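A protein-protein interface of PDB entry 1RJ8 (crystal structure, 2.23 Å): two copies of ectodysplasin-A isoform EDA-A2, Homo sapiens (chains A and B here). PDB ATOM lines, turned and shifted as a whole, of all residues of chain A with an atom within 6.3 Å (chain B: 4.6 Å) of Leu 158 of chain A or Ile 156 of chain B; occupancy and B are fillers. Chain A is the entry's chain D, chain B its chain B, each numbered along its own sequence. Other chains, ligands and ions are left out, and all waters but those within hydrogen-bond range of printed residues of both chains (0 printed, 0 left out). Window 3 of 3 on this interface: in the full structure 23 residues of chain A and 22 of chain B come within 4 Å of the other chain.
N of Phe 77 of chain A lies within hydrogen-bond range of O of Ile 156 of chain A (2.8 Å).
The backbone carbonyl oxygen (O) of Phe 77 of chain B is in hydrogen-bond range of the backbone NH (N) of Ile 156 of chain B, 2.8 Å away.
OG1 of Thr 75 of chain A lies within hydrogen-bond range of O of Glu 160 of chain A, 2.7 Å away.
The backbone NH (N) of Leu 158 of chain A is in hydrogen-bond range of the backbone carbonyl oxygen (O) of Thr 75 of chain A (2.9 Å).
The backbone NH (N) of Thr 75 of chain A sits at hydrogen-bond distance from the backbone carbonyl oxygen (O) of Gly 159 of chain A (3.0 Å).
Printed residues of chain B within 4 Å of Phe 77 of chain A: Phe 77 (3.97 Å).
Leu 158 of chain A touches just these residues of chain B: Pro 23 (3.5 Å) and Ile 156 (3.8 Å).
Glu 160 of chain A touches none of the printed residues of chain B.
Printed residues of chain A within 4 Å of Pro 23 of chain B: Leu 158 (3.5 Å).
Thr 75 of chain B touches none of the printed residues of chain A.
Of the printed residues of chain A, Ile 156 of chain B touches Leu 158 (3.8 Å).
Among the printed residues, pairs that only touch across the chains: Thr 75 of chain A with Val 25 of chain B (3.7 Å), Phe 77 of chain A with Phe 77 of chain B (3.97 Å), Val 124 of chain A with Val 25 of chain B (3.97 Å), Leu 158 of chain A with Pro 23 of chain B (3.5 Å) and Leu 158 of chain A with Ile 156 of chain B (3.8 Å).
Phe 77 of chain B touches its own counterpart, Phe 77 of chain A.
Leu 158 of chain A touches Pro 23 of chain B, but with the chains exchanged Pro 23 of chain A does not touch Leu 158 of chain B (7.9 Å).
Leu 158 of chain A touches Ile 156 of chain B, but with the chains exchanged Ile 156 of chain A does not touch Leu 158 of chain B (7.9 Å).
Of the 5 pairs that touch across the chains among the printed residues, 1 has its exchanged pair printed and touching as well.
Printed residues of chain A that touch a printed residue of chain B: Thr 75, Phe 77, Val 124 and Leu 158.
Hydrophobic or aromatic side chains of chain A within 4 Å of the printed part of chain B: Phe 77, Val 124 and Leu 158.
Hydrophobic or aromatic side chains of chain B within 4 Å of the printed part of chain A: Pro 23, Val 25, Phe 77 and Ile 156.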
ATOM      1  N   PRO A  23      19.824  -4.587 -24.296  1.00  0.00           N
ATOM      2  CA  PRO A  23      18.914  -4.155 -23.195  1.00  0.00           C
ATOM      3  C   PRO A  23      17.822  -3.160 -23.626  1.00  0.00           C
ATOM      4  O   PRO A  23      18.076  -2.238 -24.406  1.00  0.00           O
ATOM      5  CB  PRO A  23      19.875  -3.504 -22.192  1.00  0.00           C
ATOM      6  CG  PRO A  23      21.179  -4.216 -22.402  1.00  0.00           C
ATOM      7  CD  PRO A  23      21.240  -4.516 -23.885  1.00  0.00           C
ATOM      8  N   ALA A  24      16.616  -3.372 -23.107  1.00  0.00           N
ATOM      9  CA  ALA A  24      15.474  -2.485 -23.322  1.00  0.00           C
ATOM     10  C   ALA A  24      15.385  -1.501 -22.167  1.00  0.00           C
ATOM     11  O   ALA A  24      15.638  -1.874 -21.021  1.00  0.00           O
ATOM     12  CB  ALA A  24      14.206  -3.297 -23.401  1.00  0.00           C
ATOM     13  N   THR A  75      15.976  -9.497 -15.307  1.00  0.00           N
ATOM     14  CA  THR A  75      16.736  -8.764 -14.309  1.00  0.00           C
ATOM     15  C   THR A  75      16.599  -7.281 -14.628  1.00  0.00           C
ATOM     16  O   THR A  75      17.016  -6.841 -15.696  1.00  0.00           O
ATOM     17  CB  THR A  75      18.202  -9.181 -14.400  1.00  0.00           C
ATOM     18  OG1 THR A  75      18.294 -10.610 -14.320  1.00  0.00           O
ATOM     19  CG2 THR A  75      18.988  -8.681 -13.208  1.00  0.00           C
ATOM     20  N   TYR A  76      16.008  -6.518 -13.712  1.00  0.00           N
ATOM     21  CA  TYR A  76      15.708  -5.108 -13.955  1.00  0.00           C
ATOM     22  C   TYR A  76      16.449  -4.186 -12.990  1.00  0.00           C
ATOM     23  O   TYR A  76      16.540  -4.463 -11.798  1.00  0.00           O
ATOM     24  CB  TYR A  76      14.202  -4.861 -13.858  1.00  0.00           C
ATOM     25  CG  TYR A  76      13.410  -5.452 -15.004  1.00  0.00           C
ATOM     26  CD1 TYR A  76      12.909  -6.750 -14.938  1.00  0.00           C
ATOM     27  CD2 TYR A  76      13.166  -4.717 -16.160  1.00  0.00           C
ATOM     28  CE1 TYR A  76      12.181  -7.297 -15.986  1.00  0.00           C
ATOM     29  CE2 TYR A  76      12.437  -5.261 -17.217  1.00  0.00           C
ATOM     30  CZ  TYR A  76      11.949  -6.552 -17.124  1.00  0.00           C
ATOM     31  OH  TYR A  76      11.227  -7.089 -18.174  1.00  0.00           O
ATOM     32  N   PHE A  77      17.006  -3.103 -13.527  1.00  0.00           N
ATOM     33  CA  PHE A  77      17.512  -1.995 -12.733  1.00  0.00           C
ATOM     34  C   PHE A  77      16.393  -0.976 -12.724  1.00  0.00           C
ATOM     35  O   PHE A  77      15.854  -0.646 -13.770  1.00  0.00           O
ATOM     36  CB  PHE A  77      18.771  -1.394 -13.365  1.00  0.00           C
ATOM     37  CG  PHE A  77      19.395  -0.290 -12.548  1.00  0.00           C
ATOM     38  CD1 PHE A  77      20.064  -0.582 -11.370  1.00  0.00           C
ATOM     39  CD2 PHE A  77      19.317   1.035 -12.953  1.00  0.00           C
ATOM     40  CE1 PHE A  77      20.641   0.417 -10.608  1.00  0.00           C
ATOM     41  CE2 PHE A  77      19.906   2.045 -12.186  1.00  0.00           C
ATOM     42  CZ  PHE A  77      20.565   1.726 -11.016  1.00  0.00           C
ATOM     43  N   VAL A 124      18.442  -3.063  -8.086  1.00  0.00           N
ATOM     44  CA  VAL A 124      18.279  -4.129  -9.056  1.00  0.00           C
ATOM     45  C   VAL A 124      17.448  -5.251  -8.426  1.00  0.00           C
ATOM     46  O   VAL A 124      17.575  -5.539  -7.240  1.00  0.00           O
ATOM     47  CB  VAL A 124      19.666  -4.633  -9.577  1.00  0.00           C
ATOM     48  CG1 VAL A 124      20.285  -5.642  -8.645  1.00  0.00           C
ATOM     49  CG2 VAL A 124      19.533  -5.230 -10.966  1.00  0.00           C
ATOM     50  N   ILE A 156      15.853  -0.430 -16.628  1.00  0.00           N
ATOM     51  CA  ILE A 156      16.662  -1.092 -17.628  1.00  0.00           C
ATOM     52  C   ILE A 156      16.515  -2.593 -17.426  1.00  0.00           C
ATOM     53  O   ILE A 156      16.837  -3.107 -16.356  1.00  0.00           O
ATOM     54  CB  ILE A 156      18.160  -0.747 -17.453  1.00  0.00           C
ATOM     55  CG1 ILE A 156      18.415   0.765 -17.445  1.00  0.00           C
ATOM     56  CG2 ILE A 156      18.971  -1.406 -18.542  1.00  0.00           C
ATOM     57  CD1 ILE A 156      19.794   1.140 -16.864  1.00  0.00           C
ATOM     58  N   ARG A 157      16.025  -3.293 -18.443  1.00  0.00           N
ATOM     59  CA  ARG A 157      16.134  -4.743 -18.479  1.00  0.00           C
ATOM     60  C   ARG A 157      17.552  -5.125 -18.874  1.00  0.00           C
ATOM     61  O   ARG A 157      17.892  -5.132 -20.054  1.00  0.00           O
ATOM     62  CB  ARG A 157      15.153  -5.337 -19.476  1.00  0.00           C
ATOM     63  CG  ARG A 157      15.055  -6.827 -19.369  1.00  0.00           C
ATOM     64  CD  ARG A 157      14.101  -7.449 -20.355  1.00  0.00           C
ATOM     65  NE  ARG A 157      14.044  -8.892 -20.164  1.00  0.00           N
ATOM     66  CZ  ARG A 157      14.785  -9.786 -20.809  1.00  0.00           C
ATOM     67  NH1 ARG A 157      15.668  -9.415 -21.729  1.00  0.00           N
ATOM     68  NH2 ARG A 157      14.640 -11.076 -20.532  1.00  0.00           N
ATOM     69  N   LEU A 158      18.374  -5.431 -17.878  1.00  0.00           N
ATOM     70  CA  LEU A 158      19.773  -5.788 -18.094  1.00  0.00           C
ATOM     71  C   LEU A 158      19.930  -7.120 -18.830  1.00  0.00           C
ATOM     72  O   LEU A 158      20.936  -7.351 -19.494  1.00  0.00           O
ATOM     73  CB  LEU A 158      20.509  -5.835 -16.752  1.00  0.00           C
ATOM     74  CG  LEU A 158      20.609  -4.472 -16.051  1.00  0.00           C
ATOM     75  CD1 LEU A 158      20.787  -4.636 -14.552  1.00  0.00           C
ATOM     76  CD2 LEU A 158      21.739  -3.646 -16.643  1.00  0.00           C
ATOM     77  N   GLY A 159      18.927  -7.985 -18.711  1.00  0.00           N
ATOM     78  CA  GLY A 159      18.936  -9.279 -19.370  1.00  0.00           C
ATOM     79  C   GLY A 159      17.894 -10.233 -18.809  1.00  0.00           C
ATOM     80  O   GLY A 159      16.921  -9.814 -18.185  1.00  0.00           O
ATOM     81  N   GLU A 160      18.092 -11.523 -19.047  1.00  0.00           N
ATOM     82  CA  GLU A 160      17.192 -12.535 -18.508  1.00  0.00           C
ATOM     83  C   GLU A 160      17.390 -12.693 -16.996  1.00  0.00           C
ATOM     84  O   GLU A 160      18.428 -12.306 -16.453  1.00  0.00           O
ATOM     85  CB  GLU A 160      17.404 -13.878 -19.219  1.00  0.00           C
ATOM     86  CG  GLU A 160      18.729 -14.571 -18.915  1.00  0.00           C
ATOM     87  CD  GLU A 160      18.902 -15.877 -19.669  1.00  0.00           C
ATOM     88  OE1 GLU A 160      17.944 -16.315 -20.350  1.00  0.00           O
ATOM     89  OE2 GLU A 160      20.002 -16.472 -19.582  1.00  0.00           O
ATOM     90  N   PRO B  23      23.982 -11.069 -17.423  1.00  0.00           N
ATOM     91  CA  PRO B  23      24.565 -10.315 -16.277  1.00  0.00           C
ATOM     92  C   PRO B  23      24.190 -10.896 -14.910  1.00  0.00           C
ATOM     93  O   PRO B  23      23.016 -11.134 -14.632  1.00  0.00           O
ATOM     94  CB  PRO B  23      23.970  -8.913 -16.449  1.00  0.00           C
ATOM     95  CG  PRO B  23      23.747  -8.776 -17.930  1.00  0.00           C
ATOM     96  CD  PRO B  23      23.467 -10.158 -18.464  1.00  0.00           C
ATOM     97  N   ALA B  24      25.201 -11.132 -14.081  1.00  0.00           N
ATOM     98  CA  ALA B  24      25.007 -11.590 -12.712  1.00  0.00           C
ATOM     99  C   ALA B  24      24.810 -10.366 -11.830  1.00  0.00           C
ATOM    100  O   ALA B  24      25.517  -9.375 -11.971  1.00  0.00           O
ATOM    101  CB  ALA B  24      26.216 -12.385 -12.242  1.00  0.00           C
ATOM    102  N   VAL B  25      23.847 -10.440 -10.924  1.00  0.00           N
ATOM    103  CA  VAL B  25      23.558  -9.335 -10.028  1.00  0.00           C
ATOM    104  C   VAL B  25      23.448  -9.812  -8.588  1.00  0.00           C
ATOM    105  O   VAL B  25      23.334 -11.006  -8.312  1.00  0.00           O
ATOM    106  CB  VAL B  25      22.246  -8.611 -10.417  1.00  0.00           C
ATOM    107  CG1 VAL B  25      22.343  -8.069 -11.828  1.00  0.00           C
ATOM    108  CG2 VAL B  25      21.038  -9.538 -10.288  1.00  0.00           C
ATOM    109  N   PHE B  59      29.258 -14.011  -7.174  1.00  0.00           N
ATOM    110  CA  PHE B  59      29.224 -13.327  -5.886  1.00  0.00           C
ATOM    111  C   PHE B  59      29.200 -14.301  -4.710  1.00  0.00           C
ATOM    112  O   PHE B  59      28.606 -15.376  -4.783  1.00  0.00           O
ATOM    113  CB  PHE B  59      28.002 -12.417  -5.827  1.00  0.00           C
ATOM    114  CG  PHE B  59      28.068 -11.263  -6.776  1.00  0.00           C
ATOM    115  CD1 PHE B  59      29.005 -10.260  -6.584  1.00  0.00           C
ATOM    116  CD2 PHE B  59      27.199 -11.171  -7.859  1.00  0.00           C
ATOM    117  CE1 PHE B  59      29.080  -9.192  -7.443  1.00  0.00           C
ATOM    118  CE2 PHE B  59      27.271 -10.096  -8.724  1.00  0.00           C
ATOM    119  CZ  PHE B  59      28.214  -9.104  -8.509  1.00  0.00           C
ATOM    120  N   THR B  75      33.756  -6.179 -15.079  1.00  0.00           N
ATOM    121  CA  THR B  75      33.294  -4.807 -14.963  1.00  0.00           C
ATOM    122  C   THR B  75      32.059  -4.833 -14.078  1.00  0.00           C
ATOM    123  O   THR B  75      31.094  -5.532 -14.387  1.00  0.00           O
ATOM    124  CB  THR B  75      32.945  -4.253 -16.357  1.00  0.00           C
ATOM    125  OG1 THR B  75      34.076  -4.396 -17.221  1.00  0.00           O
ATOM    126  CG2 THR B  75      32.711  -2.762 -16.316  1.00  0.00           C
ATOM    127  N   TYR B  76      32.099  -4.074 -12.987  1.00  0.00           N
ATOM    128  CA  TYR B  76      31.050  -4.085 -11.975  1.00  0.00           C
ATOM    129  C   TYR B  76      30.453  -2.699 -11.742  1.00  0.00           C
ATOM    130  O   TYR B  76      31.192  -1.745 -11.515  1.00  0.00           O
ATOM    131  CB  TYR B  76      31.615  -4.613 -10.656  1.00  0.00           C
ATOM    132  CG  TYR B  76      31.930  -6.086 -10.693  1.00  0.00           C
ATOM    133  CD1 TYR B  76      30.956  -7.029 -10.393  1.00  0.00           C
ATOM    134  CD2 TYR B  76      33.201  -6.541 -11.049  1.00  0.00           C
ATOM    135  CE1 TYR B  76      31.235  -8.381 -10.433  1.00  0.00           C
ATOM    136  CE2 TYR B  76      33.489  -7.894 -11.092  1.00  0.00           C
ATOM    137  CZ  TYR B  76      32.499  -8.810 -10.783  1.00  0.00           C
ATOM    138  OH  TYR B  76      32.771 -10.157 -10.821  1.00  0.00           O
ATOM    139  N   PHE B  77      29.123  -2.590 -11.823  1.00  0.00           N
ATOM    140  CA  PHE B  77      28.397  -1.447 -11.279  1.00  0.00           C
ATOM    141  C   PHE B  77      28.094  -1.729  -9.807  1.00  0.00           C
ATOM    142  O   PHE B  77      27.480  -2.734  -9.480  1.00  0.00           O
ATOM    143  CB  PHE B  77      27.092  -1.201 -12.037  1.00  0.00           C
ATOM    144  CG  PHE B  77      26.399   0.083 -11.656  1.00  0.00           C
ATOM    145  CD1 PHE B  77      27.020   1.298 -11.880  1.00  0.00           C
ATOM    146  CD2 PHE B  77      25.131   0.082 -11.085  1.00  0.00           C
ATOM    147  CE1 PHE B  77      26.412   2.485 -11.553  1.00  0.00           C
ATOM    148  CE2 PHE B  77      24.507   1.287 -10.746  1.00  0.00           C
ATOM    149  CZ  PHE B  77      25.153   2.488 -10.985  1.00  0.00           C
ATOM    150  N   ALA B 155      25.389  -5.020  -6.527  1.00  0.00           N
ATOM    151  CA  ALA B 155      26.395  -5.006  -7.577  1.00  0.00           C
ATOM    152  C   ALA B 155      25.891  -5.745  -8.810  1.00  0.00           C
ATOM    153  O   ALA B 155      25.159  -6.732  -8.702  1.00  0.00           O
ATOM    154  CB  ALA B 155      27.691  -5.634  -7.077  1.00  0.00           C
ATOM    155  N   ILE B 156      26.293  -5.251  -9.975  1.00  0.00           N
ATOM    156  CA  ILE B 156      25.962  -5.853 -11.252  1.00  0.00           C
ATOM    157  C   ILE B 156      27.265  -6.161 -11.980  1.00  0.00           C
ATOM    158  O   ILE B 156      28.082  -5.279 -12.194  1.00  0.00           O
ATOM    159  CB  ILE B 156      25.108  -4.873 -12.092  1.00  0.00           C
ATOM    160  CG1 ILE B 156      23.792  -4.544 -11.372  1.00  0.00           C
ATOM    161  CG2 ILE B 156      24.834  -5.445 -13.489  1.00  0.00           C
ATOM    162  CD1 ILE B 156      23.113  -3.307 -11.887  1.00  0.00           C
ATOM    163  N   ARG B 157      27.475  -7.420 -12.335  1.00  0.00           N
ATOM    164  CA  ARG B 157      28.553  -7.771 -13.247  1.00  0.00           C
ATOM    165  C   ARG B 157      28.084  -7.518 -14.679  1.00  0.00           C
ATOM    166  O   ARG B 157      27.366  -8.330 -15.259  1.00  0.00           O
ATOM    167  CB  ARG B 157      28.969  -9.225 -13.076  1.00  0.00           C
ATOM    168  CG  ARG B 157      30.176  -9.594 -13.908  1.00  0.00           C
ATOM    169  CD  ARG B 157      30.765 -10.940 -13.572  1.00  0.00           C
ATOM    170  NE  ARG B 157      32.027 -11.152 -14.275  1.00  0.00           N
ATOM    171  CZ  ARG B 157      32.138 -11.474 -15.564  1.00  0.00           C
ATOM    172  NH1 ARG B 157      31.063 -11.628 -16.325  1.00  0.00           N
ATOM    173  NH2 ARG B 157      33.337 -11.640 -16.105  1.00  0.00           N
ATOM    174  N   LEU B 158      28.480  -6.375 -15.228  1.00  0.00           N
ATOM    175  CA  LEU B 158      28.120  -5.988 -16.593  1.00  0.00           C
ATOM    176  C   LEU B 158      28.760  -6.906 -17.633  1.00  0.00           C
ATOM    177  O   LEU B 158      28.166  -7.191 -18.678  1.00  0.00           O
ATOM    178  CB  LEU B 158      28.510  -4.528 -16.841  1.00  0.00           C
ATOM    179  CG  LEU B 158      27.750  -3.541 -15.944  1.00  0.00           C
ATOM    180  CD1 LEU B 158      28.422  -2.177 -15.926  1.00  0.00           C
ATOM    181  CD2 LEU B 158      26.293  -3.429 -16.374  1.00  0.00           C
